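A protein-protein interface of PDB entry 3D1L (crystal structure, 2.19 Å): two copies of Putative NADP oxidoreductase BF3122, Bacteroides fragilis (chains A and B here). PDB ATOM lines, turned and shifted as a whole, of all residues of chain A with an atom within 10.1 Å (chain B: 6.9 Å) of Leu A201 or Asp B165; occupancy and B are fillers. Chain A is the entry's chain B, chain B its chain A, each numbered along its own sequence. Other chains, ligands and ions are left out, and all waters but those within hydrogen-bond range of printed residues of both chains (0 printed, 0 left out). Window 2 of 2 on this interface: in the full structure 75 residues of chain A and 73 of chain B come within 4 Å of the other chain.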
ATOM      1  N   TYR A 189      28.835 -25.379 -14.144  1.00  0.00           N
ATOM      2  CA  TYR A 189      29.079 -24.366 -13.108  1.00  0.00           C
ATOM      3  C   TYR A 189      27.831 -23.556 -12.855  1.00  0.00           C
ATOM      4  O   TYR A 189      27.545 -23.212 -11.706  1.00  0.00           O
ATOM      5  CB  TYR A 189      30.188 -23.363 -13.499  1.00  0.00           C
ATOM      6  CG  TYR A 189      31.553 -23.935 -13.857  1.00  0.00           C
ATOM      7  CD1 TYR A 189      31.950 -25.214 -13.457  1.00  0.00           C
ATOM      8  CD2 TYR A 189      32.453 -23.158 -14.578  1.00  0.00           C
ATOM      9  CE1 TYR A 189      33.195 -25.712 -13.812  1.00  0.00           C
ATOM     10  CE2 TYR A 189      33.699 -23.617 -14.915  1.00  0.00           C
ATOM     11  CZ  TYR A 189      34.073 -24.896 -14.548  1.00  0.00           C
ATOM     12  OH  TYR A 189      35.339 -25.318 -14.925  1.00  0.00           O
ATOM     13  N   ALA A 190      27.114 -23.213 -13.934  1.00  0.00           N
ATOM     14  CA  ALA A 190      25.893 -22.386 -13.851  1.00  0.00           C
ATOM     15  C   ALA A 190      24.751 -23.077 -13.108  1.00  0.00           C
ATOM     16  O   ALA A 190      24.041 -22.435 -12.337  1.00  0.00           O
ATOM     17  CB  ALA A 190      25.441 -21.951 -15.226  1.00  0.00           C
ATOM     18  N   LEU A 191      24.570 -24.372 -13.376  1.00  0.00           N
ATOM     19  CA  LEU A 191      23.583 -25.204 -12.701  1.00  0.00           C
ATOM     20  C   LEU A 191      23.921 -25.366 -11.223  1.00  0.00           C
ATOM     21  O   LEU A 191      23.051 -25.184 -10.385  1.00  0.00           O
ATOM     22  CB  LEU A 191      23.476 -26.574 -13.361  1.00  0.00           C
ATOM     23  CG  LEU A 191      22.912 -26.591 -14.785  1.00  0.00           C
ATOM     24  CD1 LEU A 191      22.921 -28.009 -15.311  1.00  0.00           C
ATOM     25  CD2 LEU A 191      21.507 -25.991 -14.816  1.00  0.00           C
ATOM     26  N   ALA A 192      25.173 -25.703 -10.914  1.00  0.00           N
ATOM     27  CA  ALA A 192      25.631 -25.744  -9.530  1.00  0.00           C
ATOM     28  C   ALA A 192      25.289 -24.424  -8.840  1.00  0.00           C
ATOM     29  O   ALA A 192      24.723 -24.452  -7.750  1.00  0.00           O
ATOM     30  CB  ALA A 192      27.118 -26.034  -9.445  1.00  0.00           C
ATOM     31  N   ALA A 193      25.596 -23.284  -9.476  1.00  0.00           N
ATOM     32  CA  ALA A 193      25.244 -21.968  -8.926  1.00  0.00           C
ATOM     33  C   ALA A 193      23.746 -21.787  -8.682  1.00  0.00           C
ATOM     34  O   ALA A 193      23.358 -21.221  -7.660  1.00  0.00           O
ATOM     35  CB  ALA A 193      25.768 -20.815  -9.815  1.00  0.00           C
ATOM     36  N   GLU A 194      22.922 -22.224  -9.639  1.00  0.00           N
ATOM     37  CA  GLU A 194      21.461 -22.145  -9.515  1.00  0.00           C
ATOM     38  C   GLU A 194      20.995 -22.903  -8.292  1.00  0.00           C
ATOM     39  O   GLU A 194      20.130 -22.430  -7.546  1.00  0.00           O
ATOM     40  CB  GLU A 194      20.754 -22.704 -10.759  1.00  0.00           C
ATOM     41  CG  GLU A 194      20.743 -21.749 -11.951  1.00  0.00           C
ATOM     42  CD  GLU A 194      19.987 -22.314 -13.155  1.00  0.00           C
ATOM     43  OE1 GLU A 194      20.310 -21.924 -14.312  1.00  0.00           O
ATOM     44  OE2 GLU A 194      19.068 -23.142 -12.946  1.00  0.00           O
ATOM     45  N   LEU A 195      21.580 -24.085  -8.118  1.00  0.00           N
ATOM     46  CA  LEU A 195      21.262 -24.974  -7.007  1.00  0.00           C
ATOM     47  C   LEU A 195      21.685 -24.366  -5.672  1.00  0.00           C
ATOM     48  O   LEU A 195      20.901 -24.338  -4.724  1.00  0.00           O
ATOM     49  CB  LEU A 195      21.934 -26.332  -7.218  1.00  0.00           C
ATOM     50  CG  LEU A 195      21.953 -27.367  -6.090  1.00  0.00           C
ATOM     51  CD1 LEU A 195      20.584 -27.983  -5.856  1.00  0.00           C
ATOM     52  CD2 LEU A 195      22.962 -28.429  -6.432  1.00  0.00           C
ATOM     53  N   LEU A 196      22.920 -23.883  -5.607  1.00  0.00           N
ATOM     54  CA  LEU A 196      23.441 -23.278  -4.388  1.00  0.00           C
ATOM     55  C   LEU A 196      22.609 -22.059  -3.961  1.00  0.00           C
ATOM     56  O   LEU A 196      22.364 -21.873  -2.769  1.00  0.00           O
ATOM     57  CB  LEU A 196      24.936 -22.940  -4.532  1.00  0.00           C
ATOM     58  CG  LEU A 196      25.928 -24.119  -4.587  1.00  0.00           C
ATOM     59  CD1 LEU A 196      27.276 -23.717  -5.165  1.00  0.00           C
ATOM     60  CD2 LEU A 196      26.114 -24.791  -3.232  1.00  0.00           C
ATOM     61  N   LYS A 197      22.154 -21.266  -4.934  1.00  0.00           N
ATOM     62  CA  LYS A 197      21.273 -20.123  -4.687  1.00  0.00           C
ATOM     63  C   LYS A 197      19.916 -20.543  -4.106  1.00  0.00           C
ATOM     64  O   LYS A 197      19.384 -19.881  -3.199  1.00  0.00           O
ATOM     65  CB  LYS A 197      21.061 -19.315  -5.978  1.00  0.00           C
ATOM     66  CG  LYS A 197      20.338 -17.970  -5.785  1.00  0.00           C
ATOM     67  CD  LYS A 197      20.215 -17.208  -7.112  1.00  0.00           C
ATOM     68  CE  LYS A 197      19.159 -16.099  -7.023  1.00  0.00           C
ATOM     69  NZ  LYS A 197      19.031 -15.398  -8.344  1.00  0.00           N
ATOM     70  N   LYS A 198      19.358 -21.636  -4.621  1.00  0.00           N
ATOM     71  CA  LYS A 198      18.107 -22.166  -4.090  1.00  0.00           C
ATOM     72  C   LYS A 198      18.246 -22.532  -2.598  1.00  0.00           C
ATOM     73  O   LYS A 198      17.256 -22.538  -1.855  1.00  0.00           O
ATOM     74  CB  LYS A 198      17.639 -23.364  -4.924  1.00  0.00           C
ATOM     75  CG  LYS A 198      16.409 -24.102  -4.363  1.00  0.00           C
ATOM     76  CD  LYS A 198      15.913 -25.167  -5.346  1.00  0.00           C
ATOM     77  CE  LYS A 198      15.062 -26.219  -4.621  1.00  0.00           C
ATOM     78  NZ  LYS A 198      14.338 -27.090  -5.598  1.00  0.00           N
ATOM     79  N   TYR A 199      19.477 -22.818  -2.175  1.00  0.00           N
ATOM     80  CA  TYR A 199      19.796 -23.156  -0.778  1.00  0.00           C
ATOM     81  C   TYR A 199      20.620 -22.075  -0.088  1.00  0.00           C
ATOM     82  O   TYR A 199      21.377 -22.364   0.840  1.00  0.00           O
ATOM     83  CB  TYR A 199      20.546 -24.482  -0.720  1.00  0.00           C
ATOM     84  CG  TYR A 199      19.662 -25.652  -1.013  1.00  0.00           C
ATOM     85  CD1 TYR A 199      18.945 -26.272   0.013  1.00  0.00           C
ATOM     86  CD2 TYR A 199      19.518 -26.125  -2.306  1.00  0.00           C
ATOM     87  CE1 TYR A 199      18.110 -27.345  -0.247  1.00  0.00           C
ATOM     88  CE2 TYR A 199      18.688 -27.204  -2.580  1.00  0.00           C
ATOM     89  CZ  TYR A 199      17.978 -27.804  -1.547  1.00  0.00           C
ATOM     90  OH  TYR A 199      17.153 -28.880  -1.805  1.00  0.00           O
ATOM     91  N   ASN A 200      20.478 -20.835  -0.552  1.00  0.00           N
ATOM     92  CA  ASN A 200      21.102 -19.668   0.093  1.00  0.00           C
ATOM     93  C   ASN A 200      22.580 -19.872   0.410  1.00  0.00           C
ATOM     94  O   ASN A 200      23.045 -19.606   1.517  1.00  0.00           O
ATOM     95  CB  ASN A 200      20.312 -19.250   1.352  1.00  0.00           C
ATOM     96  CG  ASN A 200      18.836 -19.058   1.069  1.00  0.00           C
ATOM     97  OD1 ASN A 200      17.995 -19.705   1.684  1.00  0.00           O
ATOM     98  ND2 ASN A 200      18.516 -18.203   0.101  1.00  0.00           N
ATOM     99  N   LEU A 201      23.300 -20.372  -0.592  1.00  0.00           N
ATOM    100  CA  LEU A 201      24.740 -20.569  -0.516  1.00  0.00           C
ATOM    101  C   LEU A 201      25.356 -19.948  -1.756  1.00  0.00           C
ATOM    102  O   LEU A 201      24.758 -20.018  -2.844  1.00  0.00           O
ATOM    103  CB  LEU A 201      25.085 -22.056  -0.414  1.00  0.00           C
ATOM    104  CG  LEU A 201      24.804 -22.745   0.924  1.00  0.00           C
ATOM    105  CD1 LEU A 201      24.933 -24.254   0.783  1.00  0.00           C
ATOM    106  CD2 LEU A 201      25.712 -22.219   2.027  1.00  0.00           C
ATOM    107  N   PRO A 202      26.527 -19.297  -1.591  1.00  0.00           N
ATOM    108  CA  PRO A 202      27.169 -18.650  -2.731  1.00  0.00           C
ATOM    109  C   PRO A 202      27.887 -19.660  -3.649  1.00  0.00           C
ATOM    110  O   PRO A 202      28.380 -20.702  -3.187  1.00  0.00           O
ATOM    111  CB  PRO A 202      28.159 -17.686  -2.087  1.00  0.00           C
ATOM    112  CG  PRO A 202      28.437 -18.248  -0.732  1.00  0.00           C
ATOM    113  CD  PRO A 202      27.295 -19.136  -0.342  1.00  0.00           C
ATOM    114  N   PHE A 203      27.939 -19.330  -4.937  1.00  0.00           N
ATOM    115  CA  PHE A 203      28.590 -20.175  -5.921  1.00  0.00           C
ATOM    116  C   PHE A 203      30.067 -20.372  -5.596  1.00  0.00           C
ATOM    117  O   PHE A 203      30.623 -21.433  -5.846  1.00  0.00           O
ATOM    118  CB  PHE A 203      28.429 -19.585  -7.324  1.00  0.00           C
ATOM    119  CG  PHE A 203      29.416 -20.130  -8.314  1.00  0.00           C
ATOM    120  CD1 PHE A 203      29.279 -21.444  -8.802  1.00  0.00           C
ATOM    121  CD2 PHE A 203      30.518 -19.355  -8.719  1.00  0.00           C
ATOM    122  CE1 PHE A 203      30.220 -21.963  -9.695  1.00  0.00           C
ATOM    123  CE2 PHE A 203      31.467 -19.866  -9.632  1.00  0.00           C
ATOM    124  CZ  PHE A 203      31.318 -21.172 -10.109  1.00  0.00           C
ATOM    125  N   ASP A 204      30.669 -19.343  -5.017  1.00  0.00           N
ATOM    126  CA  ASP A 204      32.107 -19.264  -4.750  1.00  0.00           C
ATOM    127  C   ASP A 204      32.718 -20.446  -4.002  1.00  0.00           C
ATOM    128  O   ASP A 204      33.921 -20.686  -4.124  1.00  0.00           O
ATOM    129  CB  ASP A 204      32.405 -17.970  -3.983  1.00  0.00           C
ATOM    130  CG  ASP A 204      31.913 -16.735  -4.722  1.00  0.00           C
ATOM    131  OD1 ASP A 204      32.598 -16.299  -5.688  1.00  0.00           O
ATOM    132  OD2 ASP A 204      30.833 -16.207  -4.342  1.00  0.00           O
ATOM    133  N   VAL A 205      31.903 -21.168  -3.226  1.00  0.00           N
ATOM    134  CA  VAL A 205      32.376 -22.342  -2.471  1.00  0.00           C
ATOM    135  C   VAL A 205      32.838 -23.476  -3.402  1.00  0.00           C
ATOM    136  O   VAL A 205      33.460 -24.450  -2.963  1.00  0.00           O
ATOM    137  CB  VAL A 205      31.300 -22.901  -1.460  1.00  0.00           C
ATOM    138  CG1 VAL A 205      30.954 -21.877  -0.404  1.00  0.00           C
ATOM    139  CG2 VAL A 205      30.021 -23.413  -2.177  1.00  0.00           C
ATOM    140  N   MET A 206      32.515 -23.333  -4.683  1.00  0.00           N
ATOM    141  CA  MET A 206      32.811 -24.339  -5.688  1.00  0.00           C
ATOM    142  C   MET A 206      34.185 -24.129  -6.314  1.00  0.00           C
ATOM    143  O   MET A 206      34.755 -25.061  -6.865  1.00  0.00           O
ATOM    144  CB  MET A 206      31.730 -24.321  -6.779  1.00  0.00           C
ATOM    145  CG  MET A 206      30.377 -24.908  -6.376  1.00  0.00           C
ATOM    146  SD  MET A 206      30.356 -26.823  -5.966  1.00  0.00           S
ATOM    147  CE  MET A 206      30.028 -26.643  -4.089  1.00  0.00           C
ATOM    148  N   PHE B 139      33.720 -23.045   5.622  1.00  0.00           N
ATOM    149  CA  PHE B 139      33.212 -23.715   6.799  1.00  0.00           C
ATOM    150  C   PHE B 139      31.707 -23.597   6.829  1.00  0.00           C
ATOM    151  O   PHE B 139      31.164 -22.507   6.614  1.00  0.00           O
ATOM    152  CB  PHE B 139      33.799 -23.105   8.068  1.00  0.00           C
ATOM    153  CG  PHE B 139      35.163 -23.614   8.405  1.00  0.00           C
ATOM    154  CD1 PHE B 139      36.266 -23.273   7.612  1.00  0.00           C
ATOM    155  CD2 PHE B 139      35.357 -24.418   9.526  1.00  0.00           C
ATOM    156  CE1 PHE B 139      37.544 -23.740   7.919  1.00  0.00           C
ATOM    157  CE2 PHE B 139      36.637 -24.895   9.852  1.00  0.00           C
ATOM    158  CZ  PHE B 139      37.736 -24.545   9.047  1.00  0.00           C
ATOM    159  N   PHE B 140      31.042 -24.711   7.120  1.00  0.00           N
ATOM    160  CA  PHE B 140      29.592 -24.726   7.184  1.00  0.00           C
ATOM    161  C   PHE B 140      29.134 -25.060   8.598  1.00  0.00           C
ATOM    162  O   PHE B 140      29.485 -26.125   9.135  1.00  0.00           O
ATOM    163  CB  PHE B 140      29.029 -25.668   6.123  1.00  0.00           C
ATOM    164  CG  PHE B 140      29.516 -25.341   4.750  1.00  0.00           C
ATOM    165  CD1 PHE B 140      28.891 -24.347   4.001  1.00  0.00           C
ATOM    166  CD2 PHE B 140      30.641 -25.972   4.229  1.00  0.00           C
ATOM    167  CE1 PHE B 140      29.362 -24.004   2.739  1.00  0.00           C
ATOM    168  CE2 PHE B 140      31.128 -25.636   2.968  1.00  0.00           C
ATOM    169  CZ  PHE B 140      30.483 -24.652   2.219  1.00  0.00           C
ATOM    170  N   ILE B 141      28.366 -24.124   9.178  1.00  0.00           N
ATOM    171  CA  ILE B 141      28.018 -24.125  10.602  1.00  0.00           C
ATOM    172  C   ILE B 141      26.523 -24.388  10.768  1.00  0.00           C
ATOM    173  O   ILE B 141      25.678 -23.778  10.071  1.00  0.00           O
ATOM    174  CB  ILE B 141      28.407 -22.764  11.307  1.00  0.00           C
ATOM    175  CG1 ILE B 141      29.869 -22.727  11.778  1.00  0.00           C
ATOM    176  CG2 ILE B 141      27.615 -22.565  12.584  1.00  0.00           C
ATOM    177  CD1 ILE B 141      30.866 -23.562  11.014  1.00  0.00           C
ATOM    178  N   GLU B 142      26.208 -25.344  11.641  1.00  0.00           N
ATOM    179  CA  GLU B 142      24.851 -25.528  12.133  1.00  0.00           C
ATOM    180  C   GLU B 142      24.995 -25.614  13.650  1.00  0.00           C
ATOM    181  O   GLU B 142      26.028 -26.104  14.151  1.00  0.00           O
ATOM    182  CB  GLU B 142      24.157 -26.770  11.529  1.00  0.00           C
ATOM    183  CG  GLU B 142      22.639 -26.751  11.718  1.00  0.00           C
ATOM    184  CD  GLU B 142      21.936 -27.983  11.175  1.00  0.00           C
ATOM    185  OE1 GLU B 142      22.596 -28.895  10.632  1.00  0.00           O
ATOM    186  OE2 GLU B 142      20.695 -28.033  11.261  1.00  0.00           O
ATOM    187  N   ALA B 143      24.006 -25.103  14.383  1.00  0.00           N
ATOM    188  CA  ALA B 143      24.041 -25.198  15.833  1.00  0.00           C
ATOM    189  C   ALA B 143      22.666 -25.290  16.476  1.00  0.00           C
ATOM    190  O   ALA B 143      21.642 -24.978  15.853  1.00  0.00           O
ATOM    191  CB  ALA B 143      24.886 -24.068  16.451  1.00  0.00           C
ATOM    192  N   ALA B 149      25.514 -20.934  17.134  1.00  0.00           N
ATOM    193  CA  ALA B 149      25.943 -20.715  15.753  1.00  0.00           C
ATOM    194  C   ALA B 149      26.917 -19.532  15.626  1.00  0.00           C
ATOM    195  O   ALA B 149      27.986 -19.671  15.016  1.00  0.00           O
ATOM    196  CB  ALA B 149      24.729 -20.549  14.807  1.00  0.00           C
ATOM    197  N   ALA B 150      26.564 -18.379  16.213  1.00  0.00           N
ATOM    198  CA  ALA B 150      27.400 -17.186  16.096  1.00  0.00           C
ATOM    199  C   ALA B 150      28.798 -17.474  16.633  1.00  0.00           C
ATOM    200  O   ALA B 150      29.791 -17.051  16.042  1.00  0.00           O
ATOM    201  CB  ALA B 150      26.772 -15.998  16.808  1.00  0.00           C
ATOM    202  N   LYS B 153      30.692 -19.735  14.265  1.00  0.00           N
ATOM    203  CA  LYS B 153      31.070 -18.920  13.106  1.00  0.00           C
ATOM    204  C   LYS B 153      32.234 -17.986  13.430  1.00  0.00           C
ATOM    205  O   LYS B 153      33.137 -17.810  12.613  1.00  0.00           O
ATOM    206  CB  LYS B 153      29.877 -18.139  12.543  1.00  0.00           C
ATOM    207  CG  LYS B 153      28.934 -18.992  11.686  1.00  0.00           C
ATOM    208  CD  LYS B 153      27.533 -18.376  11.601  1.00  0.00           C
ATOM    209  CE  LYS B 153      27.461 -17.268  10.572  1.00  0.00           C
ATOM    210  NZ  LYS B 153      26.118 -16.631  10.577  1.00  0.00           N
ATOM    211  N   VAL B 163      32.840 -18.590   5.695  1.00  0.00           N
ATOM    212  CA  VAL B 163      32.112 -19.210   6.807  1.00  0.00           C
ATOM    213  C   VAL B 163      30.615 -18.973   6.636  1.00  0.00           C
ATOM    214  O   VAL B 163      30.175 -17.819   6.526  1.00  0.00           O
ATOM    215  CB  VAL B 163      32.554 -18.667   8.196  1.00  0.00           C
ATOM    216  CG1 VAL B 163      31.801 -19.401   9.308  1.00  0.00           C
ATOM    217  CG2 VAL B 163      34.069 -18.799   8.405  1.00  0.00           C
ATOM    218  N   TYR B 164      29.845 -20.061   6.601  1.00  0.00           N
ATOM    219  CA  TYR B 164      28.432 -19.981   6.259  1.00  0.00           C
ATOM    220  C   TYR B 164      27.551 -20.784   7.189  1.00  0.00           C
ATOM    221  O   TYR B 164      28.015 -21.734   7.800  1.00  0.00           O
ATOM    222  CB  TYR B 164      28.213 -20.463   4.825  1.00  0.00           C
ATOM    223  CG  TYR B 164      29.194 -19.860   3.868  1.00  0.00           C
ATOM    224  CD1 TYR B 164      28.979 -18.590   3.332  1.00  0.00           C
ATOM    225  CD2 TYR B 164      30.360 -20.544   3.516  1.00  0.00           C
ATOM    226  CE1 TYR B 164      29.898 -18.018   2.455  1.00  0.00           C
ATOM    227  CE2 TYR B 164      31.279 -19.983   2.639  1.00  0.00           C
ATOM    228  CZ  TYR B 164      31.045 -18.728   2.121  1.00  0.00           C
ATOM    229  OH  TYR B 164      31.962 -18.188   1.253  1.00  0.00           O
ATOM    230  N   ASP B 165      26.287 -20.366   7.291  1.00  0.00           N
ATOM    231  CA  ASP B 165      25.219 -21.177   7.862  1.00  0.00           C
ATOM    232  C   ASP B 165      24.796 -22.244   6.844  1.00  0.00           C
ATOM    233  O   ASP B 165      24.611 -21.947   5.655  1.00  0.00           O
ATOM    234  CB  ASP B 165      24.004 -20.297   8.175  1.00  0.00           C
ATOM    235  CG  ASP B 165      24.235 -19.374   9.343  1.00  0.00           C
ATOM    236  OD1 ASP B 165      24.350 -19.862  10.494  1.00  0.00           O
ATOM    237  OD2 ASP B 165      24.289 -18.154   9.122  1.00  0.00           O
ATOM    238  N   ALA B 166      24.643 -23.480   7.311  1.00  0.00           N
ATOM    239  CA  ALA B 166      24.104 -24.551   6.487  1.00  0.00           C
ATOM    240  C   ALA B 166      23.565 -25.683   7.362  1.00  0.00           C
ATOM    241  O   ALA B 166      24.284 -26.229   8.201  1.00  0.00           O
ATOM    242  CB  ALA B 166      25.169 -25.089   5.514  1.00  0.00           C
ATOM    243  N   ASP B 167      22.303 -26.029   7.143  1.00  0.00           N
ATOM    244  CA  ASP B 167      21.691 -27.198   7.766  1.00  0.00           C
ATOM    245  C   ASP B 167      21.961 -28.461   6.945  1.00  0.00           C
ATOM    246  O   ASP B 167      22.687 -28.397   5.966  1.00  0.00           O
ATOM    247  CB  ASP B 167      20.195 -26.966   8.004  1.00  0.00           C
ATOM    248  CG  ASP B 167      19.429 -26.598   6.745  1.00  0.00           C
ATOM    249  OD1 ASP B 167      18.381 -25.932   6.922  1.00  0.00           O
ATOM    250  OD2 ASP B 167      19.825 -26.984   5.607  1.00  0.00           O
ATOM    251  N   GLU B 169      20.179 -30.188   4.837  1.00  0.00           N
ATOM    252  CA  GLU B 169      19.635 -30.014   3.479  1.00  0.00           C
ATOM    253  C   GLU B 169      20.538 -29.154   2.599  1.00  0.00           C
ATOM    254  O   GLU B 169      20.802 -29.488   1.438  1.00  0.00           O
ATOM    255  CB  GLU B 169      18.239 -29.389   3.573  1.00  0.00           C
ATOM    256  CG  GLU B 169      17.314 -29.688   2.417  1.00  0.00           C
ATOM    257  CD  GLU B 169      16.997 -31.167   2.272  1.00  0.00           C
ATOM    258  OE1 GLU B 169      16.873 -31.857   3.323  1.00  0.00           O
ATOM    259  OE2 GLU B 169      16.866 -31.622   1.099  1.00  0.00           O
ATOM    260  N   GLN B 170      21.001 -28.045   3.165  1.00  0.00           N
ATOM    261  CA  GLN B 170      22.006 -27.193   2.546  1.00  0.00           C
ATOM    262  C   GLN B 170      23.332 -27.922   2.370  1.00  0.00           C
ATOM    263  O   GLN B 170      24.017 -27.723   1.374  1.00  0.00           O
ATOM    264  CB  GLN B 170      22.223 -25.927   3.378  1.00  0.00           C
ATOM    265  CG  GLN B 170      21.066 -24.968   3.326  1.00  0.00           C
ATOM    266  CD  GLN B 170      21.213 -23.819   4.303  1.00  0.00           C
ATOM    267  OE1 GLN B 170      21.074 -23.996   5.516  1.00  0.00           O
ATOM    268  NE2 GLN B 170      21.465 -22.622   3.775  1.00  0.00           N
ATOM    269  N   ARG B 171      23.705 -28.764   3.330  1.00  0.00           N
ATOM    270  CA  ARG B 171      24.968 -29.499   3.204  1.00  0.00           C
ATOM    271  C   ARG B 171      24.870 -30.562   2.118  1.00  0.00           C
ATOM    272  O   ARG B 171      25.824 -30.759   1.373  1.00  0.00           O
ATOM    273  CB  ARG B 171      25.415 -30.090   4.530  1.00  0.00           C
ATOM    274  CG  ARG B 171      25.890 -29.043   5.514  1.00  0.00           C
ATOM    275  CD  ARG B 171      26.648 -29.681   6.703  1.00  0.00           C
ATOM    276  NE  ARG B 171      25.870 -30.718   7.379  1.00  0.00           N
ATOM    277  CZ  ARG B 171      24.990 -30.513   8.360  1.00  0.00           C
ATOM    278  NH1 ARG B 171      24.734 -29.284   8.809  1.00  0.00           N
ATOM    279  NH2 ARG B 171      24.338 -31.545   8.882  1.00  0.00           N
ATOM    280  N   SER B 173      23.092 -30.186  -0.570  1.00  0.00           N
ATOM    281  CA  SER B 173      23.169 -29.420  -1.804  1.00  0.00           C
ATOM    282  C   SER B 173      24.614 -29.143  -2.254  1.00  0.00           C
ATOM    283  O   SER B 173      24.886 -29.073  -3.459  1.00  0.00           O
ATOM    284  CB  SER B 173      22.332 -28.130  -1.728  1.00  0.00           C
ATOM    285  OG  SER B 173      23.055 -27.079  -1.117  1.00  0.00           O
ATOM    286  N   LEU B 174      25.531 -28.998  -1.297  1.00  0.00           N
ATOM    287  CA  LEU B 174      26.960 -28.855  -1.613  1.00  0.00           C
ATOM    288  C   LEU B 174      27.468 -30.064  -2.387  1.00  0.00           C
ATOM    289  O   LEU B 174      28.162 -29.926  -3.403  1.00  0.00           O
ATOM    290  CB  LEU B 174      27.806 -28.652  -0.341  1.00  0.00           C
ATOM    291  CG  LEU B 174      27.651 -27.381   0.506  1.00  0.00           C
ATOM    292  CD1 LEU B 174      28.327 -27.565   1.858  1.00  0.00           C
ATOM    293  CD2 LEU B 174      28.211 -26.144  -0.201  1.00  0.00           C
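Leu A201 touches just these residues of chain B: Asp B165, Gln B170, Ser B173 and Leu B174. Asp B165 touches just one residue of chain A: Leu A201 (3.8 Å). Printed residues of chain B within 4 Å of Tyr A199: Glu B169 (3.6 Å), Gln B170 (2.9 Å) and Ser B173 (3.5 Å). Of the printed residues of chain A, Phe B140 touches Val A205 (3.8 Å). Of the printed residues of chain B, Val A205 touches Phe B140, Tyr B164 and Leu B174. Glu A194 touches none of the printed residues of chain B. The nearest residue of chain A that does not touch Asp B165 is Asn A200 (5.0 Å). The nearest printed residue of chain B that does not touch Pro A202 is Phe B140 (6.1 Å).
The backbone NH of Ile B141 is in hydrogen-bond range of the backbone carbonyl oxygen of Tyr B164. NZ of Lys B153 is in salt-bridge range of OD2 of Asp B165 (2.8 Å). OD2 of Asp B167 lies close to N of Glu B169 (3.3 Å). The side-chain amide oxygen of Gln B170 lies within hydrogen-bond range of the backbone NH of Asp B167 (2.9 Å). The backbone carbonyl oxygen of Gln B170 sits at hydrogen-bond distance from the side-chain hydroxyl of Ser B173 (2.7 Å). The backbone carbonyl oxygen of Leu A196 sits at hydrogen-bond distance from the backbone NH of Leu A201 (2.8 Å).
No position is printed for both chains. Of the 14 pairs that touch across the chains among the printed residues, none has its exchanged pair printed and touching as well.
The backbone carbonyl oxygen (O) of Tyr A199 lies within hydrogen-bond range of the side-chain amide nitrogen (NE2) of Gln B170 (2.9 Å).
Printed residues of chain A that touch a printed residue of chain B: Leu A195, Leu A196, Tyr A199, Leu A201, Pro A202, Val A205 and Met A206.
Leu B174 touches Leu A196 (CD2 to CD2, 3.9 Å). Glu B169 touches Tyr A199 (CG to CE1, 3.6 Å). CB of Ser B173 touches CD2 of Tyr A199, 3.5 Å away. Asp B165 touches Leu A201. Leu A201 touches Gln B170 (CD1 to O, 3.6 Å). Leu A201 touches Ser B173 (CD1 to OG, 3.9 Å). Leu A201 touches Leu B174 (CD1 to CD2, 3.9 Å). Val A205 touches Tyr B164. CG2 of Val A205 touches CD2 of Leu B174, 3.8 Å away. CE of Met A206 touches O of Leu B174, 3.8 Å away.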
